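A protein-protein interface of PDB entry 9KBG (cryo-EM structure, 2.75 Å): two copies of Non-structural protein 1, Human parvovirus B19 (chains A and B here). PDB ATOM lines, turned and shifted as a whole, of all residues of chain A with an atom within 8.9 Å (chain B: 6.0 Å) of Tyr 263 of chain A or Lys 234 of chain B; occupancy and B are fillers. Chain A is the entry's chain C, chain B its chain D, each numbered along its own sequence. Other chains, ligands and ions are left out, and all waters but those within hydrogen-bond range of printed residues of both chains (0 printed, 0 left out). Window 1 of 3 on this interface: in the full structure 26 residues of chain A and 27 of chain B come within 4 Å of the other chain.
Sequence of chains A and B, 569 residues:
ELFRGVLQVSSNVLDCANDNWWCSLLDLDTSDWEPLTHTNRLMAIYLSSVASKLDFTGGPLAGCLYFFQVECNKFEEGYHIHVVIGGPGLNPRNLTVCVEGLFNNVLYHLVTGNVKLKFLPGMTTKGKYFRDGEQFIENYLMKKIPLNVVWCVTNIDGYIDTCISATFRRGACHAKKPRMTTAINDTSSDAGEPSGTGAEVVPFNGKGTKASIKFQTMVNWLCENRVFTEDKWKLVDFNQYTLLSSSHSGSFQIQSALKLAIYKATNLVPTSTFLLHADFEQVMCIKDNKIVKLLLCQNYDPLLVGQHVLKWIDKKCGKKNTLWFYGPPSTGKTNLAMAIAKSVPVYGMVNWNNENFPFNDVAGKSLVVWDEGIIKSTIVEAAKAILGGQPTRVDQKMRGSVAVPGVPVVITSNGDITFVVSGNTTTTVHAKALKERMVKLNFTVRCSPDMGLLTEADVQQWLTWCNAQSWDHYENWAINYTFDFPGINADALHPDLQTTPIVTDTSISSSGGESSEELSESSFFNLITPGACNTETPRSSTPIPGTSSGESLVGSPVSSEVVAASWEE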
ATOM      1  N   VAL A 219     -14.452  31.331   5.278  1.00  0.00           N
ATOM      2  CA  VAL A 219     -14.077  31.313   6.691  1.00  0.00           C
ATOM      3  C   VAL A 219     -12.742  32.017   6.897  1.00  0.00           C
ATOM      4  O   VAL A 219     -12.577  32.810   7.835  1.00  0.00           O
ATOM      5  CB  VAL A 219     -14.043  29.865   7.215  1.00  0.00           C
ATOM      6  CG1 VAL A 219     -13.285  29.789   8.530  1.00  0.00           C
ATOM      7  CG2 VAL A 219     -15.454  29.327   7.380  1.00  0.00           C
ATOM      8  N   CYS A 223     -11.964  35.413   9.037  1.00  0.00           N
ATOM      9  CA  CYS A 223     -10.983  35.448  10.116  1.00  0.00           C
ATOM     10  C   CYS A 223      -9.935  36.536   9.908  1.00  0.00           C
ATOM     11  O   CYS A 223      -9.560  37.217  10.869  1.00  0.00           O
ATOM     12  CB  CYS A 223     -10.307  34.085  10.258  1.00  0.00           C
ATOM     13  SG  CYS A 223      -9.285  33.920  11.739  1.00  0.00           S
ATOM     14  N   PHE A 228     -16.721  39.205  12.930  1.00  0.00           N
ATOM     15  CA  PHE A 228     -17.235  38.093  13.716  1.00  0.00           C
ATOM     16  C   PHE A 228     -18.707  38.253  14.081  1.00  0.00           C
ATOM     17  O   PHE A 228     -19.224  37.445  14.863  1.00  0.00           O
ATOM     18  CB  PHE A 228     -16.406  37.913  14.996  1.00  0.00           C
ATOM     19  CG  PHE A 228     -14.933  37.749  14.746  1.00  0.00           C
ATOM     20  CD1 PHE A 228     -14.418  36.536  14.323  1.00  0.00           C
ATOM     21  CD2 PHE A 228     -14.063  38.811  14.932  1.00  0.00           C
ATOM     22  CE1 PHE A 228     -13.065  36.386  14.089  1.00  0.00           C
ATOM     23  CE2 PHE A 228     -12.711  38.666  14.700  1.00  0.00           C
ATOM     24  CZ  PHE A 228     -12.211  37.451  14.279  1.00  0.00           C
ATOM     25  N   SER A 256     -22.617  29.118  10.218  1.00  0.00           N
ATOM     26  CA  SER A 256     -21.539  28.142  10.353  1.00  0.00           C
ATOM     27  C   SER A 256     -20.175  28.809  10.213  1.00  0.00           C
ATOM     28  O   SER A 256     -19.261  28.558  11.010  1.00  0.00           O
ATOM     29  CB  SER A 256     -21.711  27.033   9.316  1.00  0.00           C
ATOM     30  OG  SER A 256     -20.771  25.995   9.518  1.00  0.00           O
ATOM     31  N   ALA A 257     -20.026  29.679   9.212  1.00  0.00           N
ATOM     32  CA  ALA A 257     -18.761  30.367   8.996  1.00  0.00           C
ATOM     33  C   ALA A 257     -18.446  31.319  10.139  1.00  0.00           C
ATOM     34  O   ALA A 257     -17.287  31.432  10.551  1.00  0.00           O
ATOM     35  CB  ALA A 257     -18.793  31.116   7.664  1.00  0.00           C
ATOM     36  N   LEU A 258     -19.457  32.019  10.664  1.00  0.00           N
ATOM     37  CA  LEU A 258     -19.211  32.910  11.793  1.00  0.00           C
ATOM     38  C   LEU A 258     -18.720  32.133  13.009  1.00  0.00           C
ATOM     39  O   LEU A 258     -17.749  32.535  13.665  1.00  0.00           O
ATOM     40  CB  LEU A 258     -20.477  33.695  12.131  1.00  0.00           C
ATOM     41  CG  LEU A 258     -20.724  34.970  11.324  1.00  0.00           C
ATOM     42  CD1 LEU A 258     -22.013  35.639  11.765  1.00  0.00           C
ATOM     43  CD2 LEU A 258     -19.552  35.924  11.454  1.00  0.00           C
ATOM     44  N   LYS A 259     -19.370  31.006  13.315  1.00  0.00           N
ATOM     45  CA  LYS A 259     -18.939  30.193  14.450  1.00  0.00           C
ATOM     46  C   LYS A 259     -17.522  29.666  14.249  1.00  0.00           C
ATOM     47  O   LYS A 259     -16.696  29.713  15.172  1.00  0.00           O
ATOM     48  CB  LYS A 259     -19.914  29.037  14.669  1.00  0.00           C
ATOM     49  CG  LYS A 259     -21.124  29.396  15.513  1.00  0.00           C
ATOM     50  CD  LYS A 259     -21.953  28.167  15.846  1.00  0.00           C
ATOM     51  CE  LYS A 259     -22.756  27.703  14.642  1.00  0.00           C
ATOM     52  NZ  LYS A 259     -23.619  26.533  14.962  1.00  0.00           N
ATOM     53  N   LEU A 260     -17.220  29.167  13.048  1.00  0.00           N
ATOM     54  CA  LEU A 260     -15.890  28.623  12.791  1.00  0.00           C
ATOM     55  C   LEU A 260     -14.821  29.704  12.879  1.00  0.00           C
ATOM     56  O   LEU A 260     -13.733  29.469  13.417  1.00  0.00           O
ATOM     57  CB  LEU A 260     -15.854  27.940  11.425  1.00  0.00           C
ATOM     58  CG  LEU A 260     -16.579  26.598  11.329  1.00  0.00           C
ATOM     59  CD1 LEU A 260     -16.420  26.007   9.942  1.00  0.00           C
ATOM     60  CD2 LEU A 260     -16.068  25.633  12.386  1.00  0.00           C
ATOM     61  N   ALA A 261     -15.108  30.898  12.352  1.00  0.00           N
ATOM     62  CA  ALA A 261     -14.145  31.990  12.424  1.00  0.00           C
ATOM     63  C   ALA A 261     -13.906  32.425  13.863  1.00  0.00           C
ATOM     64  O   ALA A 261     -12.761  32.686  14.253  1.00  0.00           O
ATOM     65  CB  ALA A 261     -14.625  33.168  11.577  1.00  0.00           C
ATOM     66  N   ILE A 262     -14.969  32.507  14.668  1.00  0.00           N
ATOM     67  CA  ILE A 262     -14.799  32.867  16.075  1.00  0.00           C
ATOM     68  C   ILE A 262     -13.934  31.832  16.784  1.00  0.00           C
ATOM     69  O   ILE A 262     -13.013  32.176  17.537  1.00  0.00           O
ATOM     70  CB  ILE A 262     -16.167  33.028  16.762  1.00  0.00           C
ATOM     71  CG1 ILE A 262     -16.894  34.263  16.231  1.00  0.00           C
ATOM     72  CG2 ILE A 262     -16.000  33.125  18.269  1.00  0.00           C
ATOM     73  CD1 ILE A 262     -18.288  34.431  16.789  1.00  0.00           C
ATOM     74  N   TYR A 263     -14.210  30.545  16.545  1.00  0.00           N
ATOM     75  CA  TYR A 263     -13.427  29.500  17.198  1.00  0.00           C
ATOM     76  C   TYR A 263     -11.966  29.552  16.771  1.00  0.00           C
ATOM     77  O   TYR A 263     -11.064  29.381  17.600  1.00  0.00           O
ATOM     78  CB  TYR A 263     -14.017  28.122  16.901  1.00  0.00           C
ATOM     79  CG  TYR A 263     -13.298  26.997  17.615  1.00  0.00           C
ATOM     80  CD1 TYR A 263     -12.206  26.361  17.036  1.00  0.00           C
ATOM     81  CD2 TYR A 263     -13.704  26.580  18.874  1.00  0.00           C
ATOM     82  CE1 TYR A 263     -11.546  25.340  17.690  1.00  0.00           C
ATOM     83  CE2 TYR A 263     -13.051  25.558  19.534  1.00  0.00           C
ATOM     84  CZ  TYR A 263     -11.973  24.943  18.937  1.00  0.00           C
ATOM     85  OH  TYR A 263     -11.319  23.925  19.592  1.00  0.00           O
ATOM     86  N   LYS A 264     -11.708  29.771  15.480  1.00  0.00           N
ATOM     87  CA  LYS A 264     -10.329  29.839  15.009  1.00  0.00           C
ATOM     88  C   LYS A 264      -9.600  31.037  15.601  1.00  0.00           C
ATOM     89  O   LYS A 264      -8.422  30.939  15.962  1.00  0.00           O
ATOM     90  CB  LYS A 264     -10.295  29.893  13.482  1.00  0.00           C
ATOM     91  CG  LYS A 264      -8.892  29.927  12.896  1.00  0.00           C
ATOM     92  CD  LYS A 264      -8.915  30.343  11.436  1.00  0.00           C
ATOM     93  CE  LYS A 264      -7.526  30.285  10.823  1.00  0.00           C
ATOM     94  NZ  LYS A 264      -7.483  30.947   9.490  1.00  0.00           N
ATOM     95  N   ALA A 265     -10.283  32.178  15.711  1.00  0.00           N
ATOM     96  CA  ALA A 265      -9.619  33.384  16.195  1.00  0.00           C
ATOM     97  C   ALA A 265      -9.357  33.320  17.695  1.00  0.00           C
ATOM     98  O   ALA A 265      -8.322  33.805  18.167  1.00  0.00           O
ATOM     99  CB  ALA A 265     -10.454  34.616  15.850  1.00  0.00           C
ATOM    100  N   THR A 266     -10.275  32.734  18.465  1.00  0.00           N
ATOM    101  CA  THR A 266     -10.179  32.802  19.918  1.00  0.00           C
ATOM    102  C   THR A 266      -9.556  31.571  20.564  1.00  0.00           C
ATOM    103  O   THR A 266      -9.277  31.606  21.767  1.00  0.00           O
ATOM    104  CB  THR A 266     -11.565  33.036  20.534  1.00  0.00           C
ATOM    105  OG1 THR A 266     -12.454  31.988  20.130  1.00  0.00           O
ATOM    106  CG2 THR A 266     -12.127  34.377  20.092  1.00  0.00           C
ATOM    107  N   ASN A 267      -9.331  30.488  19.821  1.00  0.00           N
ATOM    108  CA  ASN A 267      -8.829  29.278  20.460  1.00  0.00           C
ATOM    109  C   ASN A 267      -7.614  28.712  19.729  1.00  0.00           C
ATOM    110  O   ASN A 267      -6.711  28.153  20.359  1.00  0.00           O
ATOM    111  CB  ASN A 267      -9.951  28.236  20.538  1.00  0.00           C
ATOM    112  CG  ASN A 267      -9.582  27.023  21.380  1.00  0.00           C
ATOM    113  OD1 ASN A 267      -8.475  26.918  21.904  1.00  0.00           O
ATOM    114  ND2 ASN A 267     -10.527  26.102  21.521  1.00  0.00           N
ATOM    115  N   LEU A 268      -7.564  28.870  18.408  1.00  0.00           N
ATOM    116  CA  LEU A 268      -6.508  28.261  17.610  1.00  0.00           C
ATOM    117  C   LEU A 268      -5.357  29.208  17.300  1.00  0.00           C
ATOM    118  O   LEU A 268      -4.329  28.756  16.782  1.00  0.00           O
ATOM    119  CB  LEU A 268      -7.082  27.718  16.295  1.00  0.00           C
ATOM    120  CG  LEU A 268      -7.961  26.471  16.405  1.00  0.00           C
ATOM    121  CD1 LEU A 268      -8.363  25.983  15.026  1.00  0.00           C
ATOM    122  CD2 LEU A 268      -7.243  25.375  17.172  1.00  0.00           C
ATOM    123  N   VAL A 269      -5.496  30.496  17.593  1.00  0.00           N
ATOM    124  CA  VAL A 269      -4.447  31.471  17.302  1.00  0.00           C
ATOM    125  C   VAL A 269      -4.197  32.303  18.554  1.00  0.00           C
ATOM    126  O   VAL A 269      -5.156  32.749  19.200  1.00  0.00           O
ATOM    127  CB  VAL A 269      -4.828  32.357  16.105  1.00  0.00           C
ATOM    128  CG1 VAL A 269      -3.828  33.487  15.932  1.00  0.00           C
ATOM    129  CG2 VAL A 269      -4.913  31.527  14.835  1.00  0.00           C
ATOM    130  N   PRO A 270      -2.941  32.515  18.948  1.00  0.00           N
ATOM    131  CA  PRO A 270      -2.668  33.366  20.113  1.00  0.00           C
ATOM    132  C   PRO A 270      -3.181  34.782  19.903  1.00  0.00           C
ATOM    133  O   PRO A 270      -3.134  35.324  18.797  1.00  0.00           O
ATOM    134  CB  PRO A 270      -1.140  33.331  20.228  1.00  0.00           C
ATOM    135  CG  PRO A 270      -0.740  32.069  19.543  1.00  0.00           C
ATOM    136  CD  PRO A 270      -1.716  31.892  18.421  1.00  0.00           C
ATOM    137  N   PHE A 274      -2.676  39.168  17.017  1.00  0.00           N
ATOM    138  CA  PHE A 274      -3.541  40.239  16.542  1.00  0.00           C
ATOM    139  C   PHE A 274      -3.088  41.614  17.011  1.00  0.00           C
ATOM    140  O   PHE A 274      -3.560  42.621  16.471  1.00  0.00           O
ATOM    141  CB  PHE A 274      -4.983  39.994  16.992  1.00  0.00           C
ATOM    142  CG  PHE A 274      -5.620  38.791  16.359  1.00  0.00           C
ATOM    143  CD1 PHE A 274      -6.245  38.890  15.128  1.00  0.00           C
ATOM    144  CD2 PHE A 274      -5.594  37.561  16.994  1.00  0.00           C
ATOM    145  CE1 PHE A 274      -6.833  37.785  14.541  1.00  0.00           C
ATOM    146  CE2 PHE A 274      -6.179  36.451  16.413  1.00  0.00           C
ATOM    147  CZ  PHE A 274      -6.799  36.565  15.185  1.00  0.00           C
ATOM    148  N   VAL A 346     -12.417  39.561  19.984  1.00  0.00           N
ATOM    149  CA  VAL A 346     -13.705  39.572  20.665  1.00  0.00           C
ATOM    150  C   VAL A 346     -13.477  39.878  22.139  1.00  0.00           C
ATOM    151  O   VAL A 346     -12.510  39.397  22.740  1.00  0.00           O
ATOM    152  CB  VAL A 346     -14.454  38.231  20.502  1.00  0.00           C
ATOM    153  CG1 VAL A 346     -15.897  38.366  20.952  1.00  0.00           C
ATOM    154  CG2 VAL A 346     -14.388  37.746  19.063  1.00  0.00           C
ATOM    155  N   GLY A 364     -15.982  31.830  24.284  1.00  0.00           N
ATOM    156  CA  GLY A 364     -15.743  32.416  22.984  1.00  0.00           C
ATOM    157  C   GLY A 364     -15.161  33.811  23.006  1.00  0.00           C
ATOM    158  O   GLY A 364     -15.008  34.415  21.937  1.00  0.00           O
ATOM    159  N   LYS A 365     -14.831  34.341  24.178  1.00  0.00           N
ATOM    160  CA  LYS A 365     -14.280  35.679  24.309  1.00  0.00           C
ATOM    161  C   LYS A 365     -12.775  35.613  24.525  1.00  0.00           C
ATOM    162  O   LYS A 365     -12.243  34.625  25.037  1.00  0.00           O
ATOM    163  CB  LYS A 365     -14.936  36.427  25.473  1.00  0.00           C
ATOM    164  CG  LYS A 365     -16.455  36.432  25.435  1.00  0.00           C
ATOM    165  CD  LYS A 365     -16.977  37.189  24.227  1.00  0.00           C
ATOM    166  CE  LYS A 365     -18.469  36.983  24.052  1.00  0.00           C
ATOM    167  NZ  LYS A 365     -18.905  35.662  24.580  1.00  0.00           N
ATOM    168  N   MET A 398     -18.925  20.291  29.295  1.00  0.00           N
ATOM    169  CA  MET A 398     -19.188  20.279  27.859  1.00  0.00           C
ATOM    170  C   MET A 398     -18.010  19.706  27.079  1.00  0.00           C
ATOM    171  O   MET A 398     -18.192  18.878  26.180  1.00  0.00           O
ATOM    172  CB  MET A 398     -19.515  21.693  27.379  1.00  0.00           C
ATOM    173  CG  MET A 398     -19.599  21.837  25.868  1.00  0.00           C
ATOM    174  SD  MET A 398     -20.760  20.676  25.123  1.00  0.00           S
ATOM    175  CE  MET A 398     -20.894  21.348  23.468  1.00  0.00           C
ATOM    176  N   ARG A 399     -16.791  20.132  27.411  1.00  0.00           N
ATOM    177  CA  ARG A 399     -15.613  19.701  26.670  1.00  0.00           C
ATOM    178  C   ARG A 399     -15.010  18.405  27.196  1.00  0.00           C
ATOM    179  O   ARG A 399     -14.102  17.863  26.556  1.00  0.00           O
ATOM    180  CB  ARG A 399     -14.551  20.803  26.689  1.00  0.00           C
ATOM    181  N   VAL A 404      -9.991  23.689  30.135  1.00  0.00           N
ATOM    182  CA  VAL A 404     -10.107  23.966  28.705  1.00  0.00           C
ATOM    183  C   VAL A 404      -9.593  25.366  28.370  1.00  0.00           C
ATOM    184  O   VAL A 404      -8.725  25.496  27.495  1.00  0.00           O
ATOM    185  CB  VAL A 404     -11.552  23.772  28.215  1.00  0.00           C
ATOM    186  CG1 VAL A 404     -11.608  23.776  26.692  1.00  0.00           C
ATOM    187  CG2 VAL A 404     -12.144  22.499  28.790  1.00  0.00           C
ATOM    188  N   THR B 229     -14.795  14.205  21.104  1.00  0.00           N
ATOM    189  CA  THR B 229     -15.524  15.444  21.324  1.00  0.00           C
ATOM    190  C   THR B 229     -15.304  16.378  20.144  1.00  0.00           C
ATOM    191  O   THR B 229     -14.330  16.251  19.397  1.00  0.00           O
ATOM    192  CB  THR B 229     -15.096  16.141  22.626  1.00  0.00           C
ATOM    193  OG1 THR B 229     -13.686  16.389  22.598  1.00  0.00           O
ATOM    194  CG2 THR B 229     -15.437  15.285  23.836  1.00  0.00           C
ATOM    195  N   GLU B 230     -16.234  17.322  19.980  1.00  0.00           N
ATOM    196  CA  GLU B 230     -16.131  18.284  18.886  1.00  0.00           C
ATOM    197  C   GLU B 230     -14.911  19.180  19.049  1.00  0.00           C
ATOM    198  O   GLU B 230     -14.248  19.516  18.062  1.00  0.00           O
ATOM    199  CB  GLU B 230     -17.405  19.123  18.801  1.00  0.00           C
ATOM    200  CG  GLU B 230     -18.638  18.341  18.388  1.00  0.00           C
ATOM    201  CD  GLU B 230     -19.885  19.199  18.332  1.00  0.00           C
ATOM    202  OE1 GLU B 230     -19.817  20.379  18.736  1.00  0.00           O
ATOM    203  OE2 GLU B 230     -20.934  18.694  17.880  1.00  0.00           O
ATOM    204  N   ASP B 231     -14.605  19.586  20.284  1.00  0.00           N
ATOM    205  CA  ASP B 231     -13.449  20.445  20.519  1.00  0.00           C
ATOM    206  C   ASP B 231     -12.153  19.726  20.158  1.00  0.00           C
ATOM    207  O   ASP B 231     -11.258  20.316  19.539  1.00  0.00           O
ATOM    208  CB  ASP B 231     -13.436  20.899  21.980  1.00  0.00           C
ATOM    209  CG  ASP B 231     -12.390  21.965  22.262  1.00  0.00           C
ATOM    210  OD1 ASP B 231     -11.641  22.347  21.340  1.00  0.00           O
ATOM    211  OD2 ASP B 231     -12.320  22.426  23.422  1.00  0.00           O
ATOM    212  N   LYS B 232     -12.039  18.448  20.527  1.00  0.00           N
ATOM    213  CA  LYS B 232     -10.858  17.674  20.157  1.00  0.00           C
ATOM    214  C   LYS B 232     -10.754  17.517  18.645  1.00  0.00           C
ATOM    215  O   LYS B 232      -9.654  17.562  18.084  1.00  0.00           O
ATOM    216  CB  LYS B 232     -10.894  16.308  20.844  1.00  0.00           C
ATOM    217  CG  LYS B 232      -9.726  15.403  20.494  1.00  0.00           C
ATOM    218  CD  LYS B 232      -8.474  15.795  21.260  1.00  0.00           C
ATOM    219  CE  LYS B 232      -7.335  14.829  20.986  1.00  0.00           C
ATOM    220  NZ  LYS B 232      -7.636  13.459  21.486  1.00  0.00           N
ATOM    221  N   TRP B 233     -11.890  17.321  17.970  1.00  0.00           N
ATOM    222  CA  TRP B 233     -11.880  17.220  16.514  1.00  0.00           C
ATOM    223  C   TRP B 233     -11.411  18.522  15.874  1.00  0.00           C
ATOM    224  O   TRP B 233     -10.624  18.507  14.921  1.00  0.00           O
ATOM    225  CB  TRP B 233     -13.272  16.843  16.005  1.00  0.00           C
ATOM    226  CG  TRP B 233     -13.285  16.240  14.631  1.00  0.00           C
ATOM    227  CD1 TRP B 233     -12.288  16.288  13.701  1.00  0.00           C
ATOM    228  CD2 TRP B 233     -14.355  15.501  14.029  1.00  0.00           C
ATOM    229  NE1 TRP B 233     -12.669  15.623  12.562  1.00  0.00           N
ATOM    230  CE2 TRP B 233     -13.935  15.132  12.738  1.00  0.00           C
ATOM    231  CE3 TRP B 233     -15.628  15.116  14.460  1.00  0.00           C
ATOM    232  CZ2 TRP B 233     -14.740  14.395  11.874  1.00  0.00           C
ATOM    233  CZ3 TRP B 233     -16.426  14.387  13.601  1.00  0.00           C
ATOM    234  CH2 TRP B 233     -15.980  14.035  12.323  1.00  0.00           C
ATOM    235  N   LYS B 234     -11.889  19.661  16.383  1.00  0.00           N
ATOM    236  CA  LYS B 234     -11.439  20.948  15.863  1.00  0.00           C
ATOM    237  C   LYS B 234      -9.948  21.146  16.100  1.00  0.00           C
ATOM    238  O   LYS B 234      -9.235  21.658  15.230  1.00  0.00           O
ATOM    239  CB  LYS B 234     -12.231  22.088  16.503  1.00  0.00           C
ATOM    240  CG  LYS B 234     -13.730  22.041  16.271  1.00  0.00           C
ATOM    241  CD  LYS B 234     -14.371  23.368  16.641  1.00  0.00           C
ATOM    242  CE  LYS B 234     -15.862  23.219  16.887  1.00  0.00           C
ATOM    243  NZ  LYS B 234     -16.149  22.717  18.258  1.00  0.00           N
ATOM    244  N   LEU B 235      -9.460  20.754  17.280  1.00  0.00           N
ATOM    245  CA  LEU B 235      -8.044  20.921  17.592  1.00  0.00           C
ATOM    246  C   LEU B 235      -7.171  20.056  16.691  1.00  0.00           C
ATOM    247  O   LEU B 235      -6.207  20.544  16.089  1.00  0.00           O
ATOM    248  CB  LEU B 235      -7.789  20.588  19.062  1.00  0.00           C
ATOM    249  CG  LEU B 235      -7.957  21.722  20.075  1.00  0.00           C
ATOM    250  CD1 LEU B 235      -7.940  21.175  21.493  1.00  0.00           C
ATOM    251  CD2 LEU B 235      -6.875  22.772  19.889  1.00  0.00           C
ATOM    252  N   VAL B 236      -7.492  18.766  16.587  1.00  0.00           N
ATOM    253  CA  VAL B 236      -6.633  17.837  15.859  1.00  0.00           C
ATOM    254  C   VAL B 236      -6.725  18.078  14.356  1.00  0.00           C
ATOM    255  O   VAL B 236      -5.704  18.187  13.666  1.00  0.00           O
ATOM    256  CB  VAL B 236      -6.994  16.385  16.222  1.00  0.00           C
ATOM    257  CG1 VAL B 236      -6.487  15.425  15.159  1.00  0.00           C
ATOM    258  CG2 VAL B 236      -6.426  16.026  17.584  1.00  0.00           C
ATOM    259  N   ASP B 237      -7.945  18.172  13.825  1.00  0.00           N
ATOM    260  CA  ASP B 237      -8.177  18.270  12.382  1.00  0.00           C
ATOM    261  C   ASP B 237      -9.191  19.379  12.114  1.00  0.00           C
ATOM    262  O   ASP B 237     -10.400  19.135  12.089  1.00  0.00           O
ATOM    263  CB  ASP B 237      -8.648  16.930  11.821  1.00  0.00           C
ATOM    264  CG  ASP B 237      -8.347  16.780  10.343  1.00  0.00           C
ATOM    265  OD1 ASP B 237      -7.845  17.747   9.735  1.00  0.00           O
ATOM    266  OD2 ASP B 237      -8.613  15.694   9.789  1.00  0.00           O
ATOM    267  N   PHE B 238      -8.695  20.600  11.912  1.00  0.00           N
ATOM    268  CA  PHE B 238      -9.573  21.716  11.577  1.00  0.00           C
ATOM    269  C   PHE B 238     -10.024  21.678  10.123  1.00  0.00           C
ATOM    270  O   PHE B 238     -11.125  22.141   9.810  1.00  0.00           O
ATOM    271  CB  PHE B 238      -8.875  23.043  11.872  1.00  0.00           C
ATOM    272  CG  PHE B 238      -9.815  24.204  12.021  1.00  0.00           C
ATOM    273  CD1 PHE B 238     -10.854  24.160  12.933  1.00  0.00           C
ATOM    274  CD2 PHE B 238      -9.657  25.343  11.248  1.00  0.00           C
ATOM    275  CE1 PHE B 238     -11.719  25.227  13.071  1.00  0.00           C
ATOM    276  CE2 PHE B 238     -10.519  26.413  11.382  1.00  0.00           C
ATOM    277  CZ  PHE B 238     -11.551  26.355  12.295  1.00  0.00           C
ATOM    278  N   TYR B 241     -13.007  19.219   9.706  1.00  0.00           N
ATOM    279  CA  TYR B 241     -14.155  19.768  10.419  1.00  0.00           C
ATOM    280  C   TYR B 241     -14.761  20.944   9.661  1.00  0.00           C
ATOM    281  O   TYR B 241     -15.988  21.076   9.585  1.00  0.00           O
ATOM    282  CB  TYR B 241     -13.743  20.188  11.830  1.00  0.00           C
ATOM    283  CG  TYR B 241     -14.903  20.320  12.789  1.00  0.00           C
ATOM    284  CD1 TYR B 241     -15.333  19.237  13.542  1.00  0.00           C
ATOM    285  CD2 TYR B 241     -15.570  21.528  12.940  1.00  0.00           C
ATOM    286  CE1 TYR B 241     -16.391  19.352  14.418  1.00  0.00           C
ATOM    287  CE2 TYR B 241     -16.631  21.652  13.812  1.00  0.00           C
ATOM    288  CZ  TYR B 241     -17.037  20.562  14.550  1.00  0.00           C
ATOM    289  OH  TYR B 241     -18.093  20.680  15.423  1.00  0.00           O
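The side-chain amide nitrogen (ND2) of Asn 267 of chain A sits at hydrogen-bond distance from the side-chain hydroxyl (OH) of Tyr 263 of chain A (3.0 Å). The backbone carbonyl oxygen (O) of Lys 264 of chain A sits at hydrogen-bond distance from the backbone NH (N) of Val 269 of chain A (3.4 Å). OG1 of Thr 229 of chain B sits close to N of Lys 232 of chain B (3.4 Å).
No position is printed for both chains. Of the 9 pairs that touch across the chains among the printed residues, none has its exchanged pair printed and touching as well.
Among the printed residues, merely in contact across the chains: Tyr 263 of chain A with Lys 234 of chain B (3.5 Å), Val 404 of chain A with Asp 231 of chain B (3.6 Å), Leu 268 of chain A with Phe 238 of chain B (3.7 Å), Leu 268 of chain A with Leu 235 of chain B (3.8 Å), Asn 267 of chain A with Asp 231 of chain B (3.9 Å), Lys 264 of chain A with Phe 238 of chain B (3.9 Å), Leu 260 of chain A with Phe 238 of chain B (3.96 Å) and Arg 399 of chain A with Thr 229 of chain B (3.98 Å).
Leu 258 of chain A touches none of the printed residues of chain B. Tyr 263 of chain A touches just these residues of chain B: Asp 231 and Lys 234. Of the printed residues of chain B, Lys 264 of chain A touches Phe 238 (3.9 Å). Of the printed residues of chain B, Asn 267 of chain A touches Asp 231. Phe 274 of chain A touches none of the printed residues of chain B. Printed residues of chain B within 4 Å of Arg 399 of chain A: Thr 229. Of the printed residues of chain B, Val 404 of chain A touches Asp 231. Asp 231 of chain B touches three residues of chain A. Of chain A, only Tyr 263 (3.5 Å) comes within 4 Å of Lys 234 of chain B. Leu 235 of chain B touches one residue of chain A. The nearest residue of chain A that does not touch Lys 234 of chain B is Leu 268 of chain A (4.4 Å). The nearest printed residue of chain A that does not touch Thr 229 of chain B is Met 398 of chain A (5.1 Å).
Printed residues of chain B that touch a printed residue of chain A: Thr 229, Asp 231, Lys 234, Leu 235 and Phe 238. Hydrophobic or aromatic side chains of chain B within 4 Å of the printed part of chain A: Leu 235 and Phe 238. Printed residues of chain A that touch a printed residue of chain B: Leu 260, Tyr 263, Lys 264, Asn 267, Leu 268, Arg 399 and Val 404.
OH of Tyr 263 of chain A lies close to OD1 of Asp 231 of chain B (2.4 Å).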
